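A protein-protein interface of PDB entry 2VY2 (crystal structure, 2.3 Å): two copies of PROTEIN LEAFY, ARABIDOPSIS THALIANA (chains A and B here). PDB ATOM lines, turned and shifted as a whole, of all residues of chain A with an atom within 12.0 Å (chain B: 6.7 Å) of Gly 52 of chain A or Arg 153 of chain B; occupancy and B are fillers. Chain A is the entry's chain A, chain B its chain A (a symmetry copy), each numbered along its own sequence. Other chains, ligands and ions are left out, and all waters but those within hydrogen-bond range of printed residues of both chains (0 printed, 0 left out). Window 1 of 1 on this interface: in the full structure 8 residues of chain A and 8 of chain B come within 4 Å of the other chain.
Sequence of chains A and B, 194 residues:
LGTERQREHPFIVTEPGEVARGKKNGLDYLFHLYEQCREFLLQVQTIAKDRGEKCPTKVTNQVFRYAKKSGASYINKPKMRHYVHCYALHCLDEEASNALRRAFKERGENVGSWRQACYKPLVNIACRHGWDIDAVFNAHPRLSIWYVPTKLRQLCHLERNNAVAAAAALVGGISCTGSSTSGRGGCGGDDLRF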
ATOM      1  N   GLN A  43     -15.597  14.427  -1.443  1.00  0.00           N
ATOM      2  CA  GLN A  43     -14.320  14.988  -1.836  1.00  0.00           C
ATOM      3  C   GLN A  43     -13.741  14.315  -3.073  1.00  0.00           C
ATOM      4  O   GLN A  43     -13.056  14.964  -3.880  1.00  0.00           O
ATOM      5  CB  GLN A  43     -13.342  14.930  -0.670  1.00  0.00           C
ATOM      6  CG  GLN A  43     -13.763  15.863   0.447  1.00  0.00           C
ATOM      7  CD  GLN A  43     -12.899  15.751   1.701  1.00  0.00           C
ATOM      8  OE1 GLN A  43     -12.172  16.665   2.032  1.00  0.00           O
ATOM      9  NE2 GLN A  43     -13.008  14.651   2.409  1.00  0.00           N
ATOM     10  N   VAL A  44     -13.993  13.019  -3.222  1.00  0.00           N
ATOM     11  CA  VAL A  44     -13.496  12.298  -4.390  1.00  0.00           C
ATOM     12  C   VAL A  44     -14.319  12.719  -5.631  1.00  0.00           C
ATOM     13  O   VAL A  44     -13.786  12.813  -6.726  1.00  0.00           O
ATOM     14  CB  VAL A  44     -13.539  10.756  -4.151  1.00  0.00           C
ATOM     15  CG1 VAL A  44     -13.428   9.940  -5.476  1.00  0.00           C
ATOM     16  CG2 VAL A  44     -12.439  10.338  -3.168  1.00  0.00           C
ATOM     17  N   GLN A  45     -15.612  12.982  -5.435  1.00  0.00           N
ATOM     18  CA  GLN A  45     -16.498  13.409  -6.515  1.00  0.00           C
ATOM     19  C   GLN A  45     -16.141  14.805  -7.048  1.00  0.00           C
ATOM     20  O   GLN A  45     -16.161  15.043  -8.264  1.00  0.00           O
ATOM     21  CB  GLN A  45     -17.957  13.404  -6.041  1.00  0.00           C
ATOM     22  CG  GLN A  45     -18.513  11.988  -5.856  1.00  0.00           C
ATOM     23  CD  GLN A  45     -19.934  11.973  -5.330  1.00  0.00           C
ATOM     24  OE1 GLN A  45     -20.331  12.818  -4.515  1.00  0.00           O
ATOM     25  NE2 GLN A  45     -20.706  11.007  -5.795  1.00  0.00           N
ATOM     26  N   THR A  46     -15.822  15.703  -6.121  1.00  0.00           N
ATOM     27  CA  THR A  46     -15.390  17.045  -6.444  1.00  0.00           C
ATOM     28  C   THR A  46     -14.164  16.980  -7.369  1.00  0.00           C
ATOM     29  O   THR A  46     -14.147  17.590  -8.440  1.00  0.00           O
ATOM     30  CB  THR A  46     -15.090  17.843  -5.158  1.00  0.00           C
ATOM     31  OG1 THR A  46     -16.318  18.097  -4.462  1.00  0.00           O
ATOM     32  CG2 THR A  46     -14.435  19.194  -5.490  1.00  0.00           C
ATOM     33  N   ILE A  47     -13.162  16.199  -6.984  1.00  0.00           N
ATOM     34  CA  ILE A  47     -11.990  16.064  -7.833  1.00  0.00           C
ATOM     35  C   ILE A  47     -12.291  15.377  -9.187  1.00  0.00           C
ATOM     36  O   ILE A  47     -11.838  15.852 -10.242  1.00  0.00           O
ATOM     37  CB  ILE A  47     -10.829  15.329  -7.124  1.00  0.00           C
ATOM     38  CG1 ILE A  47     -10.496  16.014  -5.806  1.00  0.00           C
ATOM     39  CG2 ILE A  47      -9.601  15.343  -8.014  1.00  0.00           C
ATOM     40  CD1 ILE A  47     -10.259  17.546  -5.969  1.00  0.00           C
ATOM     41  N   ALA A  48     -13.032  14.261  -9.168  1.00  0.00           N
ATOM     42  CA  ALA A  48     -13.336  13.582 -10.437  1.00  0.00           C
ATOM     43  C   ALA A  48     -14.025  14.525 -11.433  1.00  0.00           C
ATOM     44  O   ALA A  48     -13.687  14.537 -12.612  1.00  0.00           O
ATOM     45  CB  ALA A  48     -14.187  12.344 -10.212  1.00  0.00           C
ATOM     46  N   LYS A  49     -14.998  15.297 -10.956  1.00  0.00           N
ATOM     47  CA  LYS A  49     -15.729  16.190 -11.823  1.00  0.00           C
ATOM     48  C   LYS A  49     -14.813  17.311 -12.346  1.00  0.00           C
ATOM     49  O   LYS A  49     -14.807  17.603 -13.538  1.00  0.00           O
ATOM     50  CB  LYS A  49     -16.976  16.749 -11.130  1.00  0.00           C
ATOM     51  CG  LYS A  49     -18.090  15.683 -10.931  1.00  0.00           C
ATOM     52  CD  LYS A  49     -19.441  16.267 -10.487  1.00  0.00           C
ATOM     53  CE  LYS A  49     -19.399  16.712  -9.042  1.00  0.00           C
ATOM     54  NZ  LYS A  49     -20.753  16.945  -8.432  1.00  0.00           N
ATOM     55  N   ASP A  50     -14.020  17.909 -11.466  1.00  0.00           N
ATOM     56  CA  ASP A  50     -13.098  18.945 -11.895  1.00  0.00           C
ATOM     57  C   ASP A  50     -12.108  18.439 -12.948  1.00  0.00           C
ATOM     58  O   ASP A  50     -11.737  19.183 -13.832  1.00  0.00           O
ATOM     59  CB  ASP A  50     -12.349  19.532 -10.708  1.00  0.00           C
ATOM     60  CG  ASP A  50     -11.697  20.867 -11.042  1.00  0.00           C
ATOM     61  OD1 ASP A  50     -12.430  21.851 -11.317  1.00  0.00           O
ATOM     62  OD2 ASP A  50     -10.450  20.915 -11.024  1.00  0.00           O
ATOM     63  N   ARG A  51     -11.705  17.172 -12.871  1.00  0.00           N
ATOM     64  CA  ARG A  51     -10.785  16.600 -13.864  1.00  0.00           C
ATOM     65  C   ARG A  51     -11.452  15.996 -15.116  1.00  0.00           C
ATOM     66  O   ARG A  51     -10.760  15.433 -15.963  1.00  0.00           O
ATOM     67  CB  ARG A  51      -9.935  15.498 -13.243  1.00  0.00           C
ATOM     68  CG  ARG A  51      -8.894  15.969 -12.238  1.00  0.00           C
ATOM     69  CD  ARG A  51      -8.198  14.766 -11.612  1.00  0.00           C
ATOM     70  NE  ARG A  51      -7.319  15.198 -10.540  1.00  0.00           N
ATOM     71  CZ  ARG A  51      -6.663  14.376  -9.728  1.00  0.00           C
ATOM     72  NH1 ARG A  51      -6.784  13.055  -9.859  1.00  0.00           N
ATOM     73  NH2 ARG A  51      -5.885  14.880  -8.782  1.00  0.00           N
ATOM     74  N   GLY A  52     -12.775  16.092 -15.232  1.00  0.00           N
ATOM     75  CA  GLY A  52     -13.481  15.344 -16.270  1.00  0.00           C
ATOM     76  C   GLY A  52     -13.179  13.836 -16.308  1.00  0.00           C
ATOM     77  O   GLY A  52     -13.085  13.249 -17.389  1.00  0.00           O
ATOM     78  N   GLU A  53     -12.979  13.216 -15.144  1.00  0.00           N
ATOM     79  CA  GLU A  53     -12.798  11.752 -15.041  1.00  0.00           C
ATOM     80  C   GLU A  53     -14.133  11.106 -14.656  1.00  0.00           C
ATOM     81  O   GLU A  53     -15.084  11.811 -14.239  1.00  0.00           O
ATOM     82  CB  GLU A  53     -11.726  11.396 -14.001  1.00  0.00           C
ATOM     83  CG  GLU A  53     -10.297  11.674 -14.488  1.00  0.00           C
ATOM     84  CD  GLU A  53      -9.228  11.574 -13.390  1.00  0.00           C
ATOM     85  OE1 GLU A  53      -9.587  11.350 -12.207  1.00  0.00           O
ATOM     86  OE2 GLU A  53      -8.020  11.729 -13.718  1.00  0.00           O
ATOM     87  N   LYS A  54     -14.264   9.789 -14.796  1.00  0.00           N
ATOM     88  CA  LYS A  54     -15.527   9.231 -14.313  1.00  0.00           C
ATOM     89  C   LYS A  54     -15.677   9.372 -12.777  1.00  0.00           C
ATOM     90  O   LYS A  54     -14.740   9.138 -12.014  1.00  0.00           O
ATOM     91  CB  LYS A  54     -15.863   7.841 -14.861  1.00  0.00           C
ATOM     92  CG  LYS A  54     -15.016   6.682 -14.409  1.00  0.00           C
ATOM     93  CD  LYS A  54     -15.694   5.372 -14.864  1.00  0.00           C
ATOM     94  CE  LYS A  54     -14.762   4.174 -14.737  1.00  0.00           C
ATOM     95  NZ  LYS A  54     -15.490   2.899 -14.969  1.00  0.00           N
ATOM     96  N   CYS A  55     -16.866   9.818 -12.385  1.00  0.00           N
ATOM     97  CA  CYS A  55     -17.232  10.199 -11.042  1.00  0.00           C
ATOM     98  C   CYS A  55     -17.987   9.068 -10.331  1.00  0.00           C
ATOM     99  O   CYS A  55     -19.087   8.726 -10.744  1.00  0.00           O
ATOM    100  CB  CYS A  55     -18.206  11.362 -11.182  1.00  0.00           C
ATOM    101  SG  CYS A  55     -18.676  12.137  -9.620  1.00  0.00           S
ATOM    102  N   PRO A  56     -17.430   8.513  -9.248  1.00  0.00           N
ATOM    103  CA  PRO A  56     -18.153   7.439  -8.532  1.00  0.00           C
ATOM    104  C   PRO A  56     -19.434   7.939  -7.876  1.00  0.00           C
ATOM    105  O   PRO A  56     -19.492   9.092  -7.445  1.00  0.00           O
ATOM    106  CB  PRO A  56     -17.180   7.005  -7.435  1.00  0.00           C
ATOM    107  CG  PRO A  56     -15.916   7.820  -7.634  1.00  0.00           C
ATOM    108  CD  PRO A  56     -16.210   8.950  -8.554  1.00  0.00           C
ATOM    109  N   THR A  57     -20.448   7.087  -7.808  1.00  0.00           N
ATOM    110  CA  THR A  57     -21.650   7.391  -7.024  1.00  0.00           C
ATOM    111  C   THR A  57     -21.788   6.547  -5.757  1.00  0.00           C
ATOM    112  O   THR A  57     -22.790   6.667  -5.072  1.00  0.00           O
ATOM    113  CB  THR A  57     -22.929   7.124  -7.826  1.00  0.00           C
ATOM    114  OG1 THR A  57     -22.807   5.841  -8.460  1.00  0.00           O
ATOM    115  CG2 THR A  57     -23.134   8.210  -8.900  1.00  0.00           C
ATOM    116  N   GLN A  62     -11.782   3.217  -4.262  1.00  0.00           N
ATOM    117  CA  GLN A  62     -11.185   4.540  -4.498  1.00  0.00           C
ATOM    118  C   GLN A  62     -11.339   5.418  -3.245  1.00  0.00           C
ATOM    119  O   GLN A  62     -10.390   6.035  -2.771  1.00  0.00           O
ATOM    120  CB  GLN A  62     -11.818   5.212  -5.757  1.00  0.00           C
ATOM    121  CG  GLN A  62     -11.099   6.494  -6.244  1.00  0.00           C
ATOM    122  CD  GLN A  62     -11.654   7.077  -7.568  1.00  0.00           C
ATOM    123  OE1 GLN A  62     -12.617   6.562  -8.161  1.00  0.00           O
ATOM    124  NE2 GLN A  62     -11.040   8.167  -8.021  1.00  0.00           N
ATOM    125  N   ILE B 133     -21.280  15.183 -20.109  1.00  0.00           N
ATOM    126  CA  ILE B 133     -21.609  14.212 -21.141  1.00  0.00           C
ATOM    127  C   ILE B 133     -22.214  12.936 -20.533  1.00  0.00           C
ATOM    128  O   ILE B 133     -23.034  12.282 -21.183  1.00  0.00           O
ATOM    129  CB  ILE B 133     -20.372  13.909 -22.041  1.00  0.00           C
ATOM    130  CG1 ILE B 133     -20.730  12.948 -23.173  1.00  0.00           C
ATOM    131  CG2 ILE B 133     -19.188  13.408 -21.207  1.00  0.00           C
ATOM    132  CD1 ILE B 133     -21.692  13.533 -24.194  1.00  0.00           C
ATOM    133  N   ASP B 134     -21.819  12.606 -19.291  1.00  0.00           N
ATOM    134  CA  ASP B 134     -22.413  11.473 -18.539  1.00  0.00           C
ATOM    135  C   ASP B 134     -23.908  11.738 -18.392  1.00  0.00           C
ATOM    136  O   ASP B 134     -24.728  10.838 -18.586  1.00  0.00           O
ATOM    137  CB  ASP B 134     -21.730  11.245 -17.165  1.00  0.00           C
ATOM    138  CG  ASP B 134     -20.290  10.743 -17.304  1.00  0.00           C
ATOM    139  OD1 ASP B 134     -20.102   9.633 -17.819  1.00  0.00           O
ATOM    140  OD2 ASP B 134     -19.325  11.449 -16.926  1.00  0.00           O
ATOM    141  N   TYR B 147     -21.621   2.796 -21.235  1.00  0.00           N
ATOM    142  CA  TYR B 147     -20.569   3.602 -20.640  1.00  0.00           C
ATOM    143  C   TYR B 147     -20.076   4.672 -21.648  1.00  0.00           C
ATOM    144  O   TYR B 147     -19.904   4.417 -22.865  1.00  0.00           O
ATOM    145  CB  TYR B 147     -19.402   2.712 -20.210  1.00  0.00           C
ATOM    146  CG  TYR B 147     -19.666   1.814 -19.022  1.00  0.00           C
ATOM    147  CD1 TYR B 147     -20.003   2.338 -17.765  1.00  0.00           C
ATOM    148  CD2 TYR B 147     -19.535   0.436 -19.143  1.00  0.00           C
ATOM    149  CE1 TYR B 147     -20.231   1.470 -16.646  1.00  0.00           C
ATOM    150  CE2 TYR B 147     -19.752  -0.411 -18.071  1.00  0.00           C
ATOM    151  CZ  TYR B 147     -20.101   0.102 -16.818  1.00  0.00           C
ATOM    152  OH  TYR B 147     -20.303  -0.789 -15.772  1.00  0.00           O
ATOM    153  N   VAL B 148     -19.872   5.875 -21.147  1.00  0.00           N
ATOM    154  CA  VAL B 148     -19.215   6.904 -21.929  1.00  0.00           C
ATOM    155  C   VAL B 148     -17.779   6.475 -22.253  1.00  0.00           C
ATOM    156  O   VAL B 148     -17.007   6.144 -21.361  1.00  0.00           O
ATOM    157  CB  VAL B 148     -19.200   8.228 -21.177  1.00  0.00           C
ATOM    158  CG1 VAL B 148     -18.363   9.256 -21.939  1.00  0.00           C
ATOM    159  CG2 VAL B 148     -20.626   8.735 -21.009  1.00  0.00           C
ATOM    160  N   PRO B 149     -17.423   6.448 -23.546  1.00  0.00           N
ATOM    161  CA  PRO B 149     -16.040   6.092 -23.926  1.00  0.00           C
ATOM    162  C   PRO B 149     -15.046   7.155 -23.407  1.00  0.00           C
ATOM    163  O   PRO B 149     -15.362   8.355 -23.421  1.00  0.00           O
ATOM    164  CB  PRO B 149     -16.062   6.065 -25.466  1.00  0.00           C
ATOM    165  CG  PRO B 149     -17.412   6.492 -25.880  1.00  0.00           C
ATOM    166  CD  PRO B 149     -18.277   6.822 -24.684  1.00  0.00           C
ATOM    167  N   THR B 150     -13.888   6.701 -22.919  1.00  0.00           N
ATOM    168  CA  THR B 150     -12.847   7.578 -22.365  1.00  0.00           C
ATOM    169  C   THR B 150     -12.431   8.732 -23.296  1.00  0.00           C
ATOM    170  O   THR B 150     -12.407   9.893 -22.888  1.00  0.00           O
ATOM    171  CB  THR B 150     -11.562   6.795 -22.035  1.00  0.00           C
ATOM    172  OG1 THR B 150     -11.885   5.625 -21.284  1.00  0.00           O
ATOM    173  CG2 THR B 150     -10.622   7.659 -21.221  1.00  0.00           C
ATOM    174  N   LYS B 151     -12.089   8.394 -24.534  1.00  0.00           N
ATOM    175  CA  LYS B 151     -11.684   9.395 -25.504  1.00  0.00           C
ATOM    176  C   LYS B 151     -12.728  10.497 -25.578  1.00  0.00           C
ATOM    177  O   LYS B 151     -12.385  11.684 -25.543  1.00  0.00           O
ATOM    178  CB  LYS B 151     -11.422   8.772 -26.896  1.00  0.00           C
ATOM    179  CG  LYS B 151     -11.136   9.812 -28.007  1.00  0.00           C
ATOM    180  N   LEU B 152     -14.007  10.129 -25.639  1.00  0.00           N
ATOM    181  CA  LEU B 152     -15.031  11.165 -25.725  1.00  0.00           C
ATOM    182  C   LEU B 152     -15.065  12.023 -24.453  1.00  0.00           C
ATOM    183  O   LEU B 152     -15.229  13.255 -24.530  1.00  0.00           O
ATOM    184  CB  LEU B 152     -16.407  10.572 -26.009  1.00  0.00           C
ATOM    185  CG  LEU B 152     -17.582  11.549 -25.903  1.00  0.00           C
ATOM    186  CD1 LEU B 152     -17.492  12.656 -26.952  1.00  0.00           C
ATOM    187  CD2 LEU B 152     -18.900  10.805 -26.046  1.00  0.00           C
ATOM    188  N   ARG B 153     -14.915  11.385 -23.285  1.00  0.00           N
ATOM    189  CA  ARG B 153     -14.914  12.159 -22.032  1.00  0.00           C
ATOM    190  C   ARG B 153     -13.733  13.149 -22.001  1.00  0.00           C
ATOM    191  O   ARG B 153     -13.892  14.287 -21.574  1.00  0.00           O
ATOM    192  CB  ARG B 153     -14.899  11.265 -20.778  1.00  0.00           C
ATOM    193  CG  ARG B 153     -15.239  12.036 -19.501  1.00  0.00           C
ATOM    194  CD  ARG B 153     -15.183  11.179 -18.235  1.00  0.00           C
ATOM    195  NE  ARG B 153     -16.408  10.409 -17.984  1.00  0.00           N
ATOM    196  CZ  ARG B 153     -16.468   9.098 -18.142  1.00  0.00           C
ATOM    197  NH1 ARG B 153     -15.387   8.456 -18.572  1.00  0.00           N
ATOM    198  NH2 ARG B 153     -17.590   8.431 -17.876  1.00  0.00           N
ATOM    199  N   GLN B 154     -12.562  12.699 -22.457  1.00  0.00           N
ATOM    200  CA  GLN B 154     -11.389  13.555 -22.584  1.00  0.00           C
ATOM    201  C   GLN B 154     -11.633  14.752 -23.507  1.00  0.00           C
ATOM    202  O   GLN B 154     -11.352  15.882 -23.116  1.00  0.00           O
ATOM    203  CB  GLN B 154     -10.177  12.747 -23.047  1.00  0.00           C
ATOM    204  CG  GLN B 154      -9.581  11.889 -21.935  1.00  0.00           C
ATOM    205  CD  GLN B 154      -8.658  10.786 -22.466  1.00  0.00           C
ATOM    206  OE1 GLN B 154      -8.520  10.597 -23.689  1.00  0.00           O
ATOM    207  NE2 GLN B 154      -8.025  10.045 -21.545  1.00  0.00           N
ATOM    208  N   LEU B 155     -12.177  14.522 -24.702  1.00  0.00           N
ATOM    209  CA  LEU B 155     -12.479  15.629 -25.613  1.00  0.00           C
ATOM    210  C   LEU B 155     -13.415  16.664 -24.999  1.00  0.00           C
ATOM    211  O   LEU B 155     -13.214  17.870 -25.180  1.00  0.00           O
ATOM    212  CB  LEU B 155     -13.019  15.146 -26.974  1.00  0.00           C
ATOM    213  CG  LEU B 155     -12.073  14.150 -27.665  1.00  0.00           C
ATOM    214  CD1 LEU B 155     -12.672  13.579 -28.944  1.00  0.00           C
ATOM    215  CD2 LEU B 155     -10.718  14.805 -27.954  1.00  0.00           C
ATOM    216  N   CYS B 156     -14.434  16.220 -24.268  1.00  0.00           N
ATOM    217  CA  CYS B 156     -15.379  17.182 -23.682  1.00  0.00           C
ATOM    218  C   CYS B 156     -14.693  18.045 -22.614  1.00  0.00           C
ATOM    219  O   CYS B 156     -15.012  19.224 -22.438  1.00  0.00           O
ATOM    220  CB  CYS B 156     -16.614  16.475 -23.099  1.00  0.00           C
ATOM    221  SG  CYS B 156     -17.758  15.789 -24.356  1.00  0.00           S
ATOM    222  N   HIS B 157     -13.740  17.446 -21.913  1.00  0.00           N
ATOM    223  CA  HIS B 157     -13.028  18.143 -20.851  1.00  0.00           C
ATOM    224  C   HIS B 157     -12.017  19.150 -21.442  1.00  0.00           C
ATOM    225  O   HIS B 157     -11.962  20.306 -21.029  1.00  0.00           O
ATOM    226  CB  HIS B 157     -12.336  17.120 -19.949  1.00  0.00           C
ATOM    227  CG  HIS B 157     -11.531  17.726 -18.836  1.00  0.00           C
ATOM    228  ND1 HIS B 157     -12.110  18.370 -17.762  1.00  0.00           N
ATOM    229  CD2 HIS B 157     -10.191  17.758 -18.619  1.00  0.00           C
ATOM    230  CE1 HIS B 157     -11.160  18.775 -16.934  1.00  0.00           C
ATOM    231  NE2 HIS B 157      -9.987  18.413 -17.429  1.00  0.00           N
ATOM    232  N   LEU B 158     -11.232  18.689 -22.408  1.00  0.00           N
ATOM    233  CA  LEU B 158     -10.317  19.538 -23.157  1.00  0.00           C
ATOM    234  C   LEU B 158     -11.053  20.764 -23.697  1.00  0.00           C
ATOM    235  O   LEU B 158     -10.632  21.905 -23.499  1.00  0.00           O
ATOM    236  CB  LEU B 158      -9.694  18.739 -24.303  1.00  0.00           C
ATOM    237  CG  LEU B 158      -8.709  19.484 -25.212  1.00  0.00           C
ATOM    238  CD1 LEU B 158      -7.646  20.185 -24.372  1.00  0.00           C
ATOM    239  CD2 LEU B 158      -8.053  18.561 -26.249  1.00  0.00           C
ATOM    240  N   ARG B 160     -13.958  22.031 -22.661  1.00  0.00           N
ATOM    241  CA  ARG B 160     -14.472  22.912 -21.608  1.00  0.00           C
ATOM    242  C   ARG B 160     -13.366  23.832 -21.073  1.00  0.00           C
ATOM    243  O   ARG B 160     -13.601  24.986 -20.739  1.00  0.00           O
ATOM    244  CB  ARG B 160     -15.075  22.101 -20.459  1.00  0.00           C
ATOM    245  CG  ARG B 160     -15.746  22.959 -19.392  1.00  0.00           C
ATOM    246  CD  ARG B 160     -16.104  22.168 -18.132  1.00  0.00           C
ATOM    247  NE  ARG B 160     -14.943  21.578 -17.456  1.00  0.00           N
ATOM    248  CZ  ARG B 160     -14.136  22.239 -16.623  1.00  0.00           C
ATOM    249  NH1 ARG B 160     -14.353  23.525 -16.373  1.00  0.00           N
ATOM    250  NH2 ARG B 160     -13.107  21.621 -16.039  1.00  0.00           N
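No position is printed for both chains.
Of the 7 pairs that touch across the chains among the printed residues, none has its exchanged pair printed and touching as well.
The backbone carbonyl oxygen (O) of Arg 51 of chain A is in hydrogen-bond range of a ring nitrogen (NE2) of His 157 of chain B (3.4 Å).
The backbone NH (N) of Gly 52 of chain A sits at hydrogen-bond distance from a ring nitrogen (ND1) of His 157 of chain B (3.5 Å).
Gly 52 of chain A touches just these residues of chain B: Arg 153 (3.1 Å) and His 157 (3.5 Å).
Of chain A, only Gly 52, Glu 53 and Lys 54 come within 4 Å of Arg 153 of chain B.
No residue of chain A comes within 4 Å of Val 148 of chain B.
No residue of chain A comes within 4 Å of Pro 149 of chain B.
No residue of chain A comes within 4 Å of Leu 152 of chain B.
No residue of chain A comes within 4 Å of Gln 154 of chain B.
No residue of chain A comes within 4 Å of Cys 156 of chain B.
Printed residues of chain A within 4 Å of Arg 160 of chain B: Asp 50.
Printed residues of chain B within 4 Å of Arg 51 of chain A: His 157 (3.3 Å).
Of the printed residues of chain B, Lys 54 of chain A touches Arg 153 (3.5 Å).
Of the printed residues of chain B, Asp 50 of chain A touches His 157 (3.2 Å) and Arg 160 (3.6 Å).
Printed residues of chain B within 4 Å of Glu 53 of chain A: Arg 153.
The nearest residue of chain B that does not touch Gly 52 of chain A is Gln 154 of chain B (5.1 Å).
The backbone carbonyl oxygen of Ala 48 of chain A sits at hydrogen-bond distance from the backbone NH of Glu 53 of chain A (2.9 Å).
The side-chain carboxylate (OD1) of Asp 134 of chain B is in salt-bridge range of the guanidinium group (NH2) of Arg 153 of chain B, at 2.8 Å.
Among the printed residues, merely in contact across the chains: Asp 50 of chain A with His 157 of chain B, Asp 50 of chain A with Arg 160 of chain B, Gly 52 of chain A with Arg 153 of chain B, Glu 53 of chain A with Arg 153 of chain B and Lys 54 of chain A with Arg 153 of chain B.
Of the 15 printed residues of chain B, 3 touch a printed residue of chain A.
Hydrophobic or aromatic side chains of chain B within 4 Å of the printed part of chain A: His 157.
Among the printed residues, no Asp or Glu carboxylate lies within 4 Å of a Lys or Arg side-chain nitrogen of the other chain.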
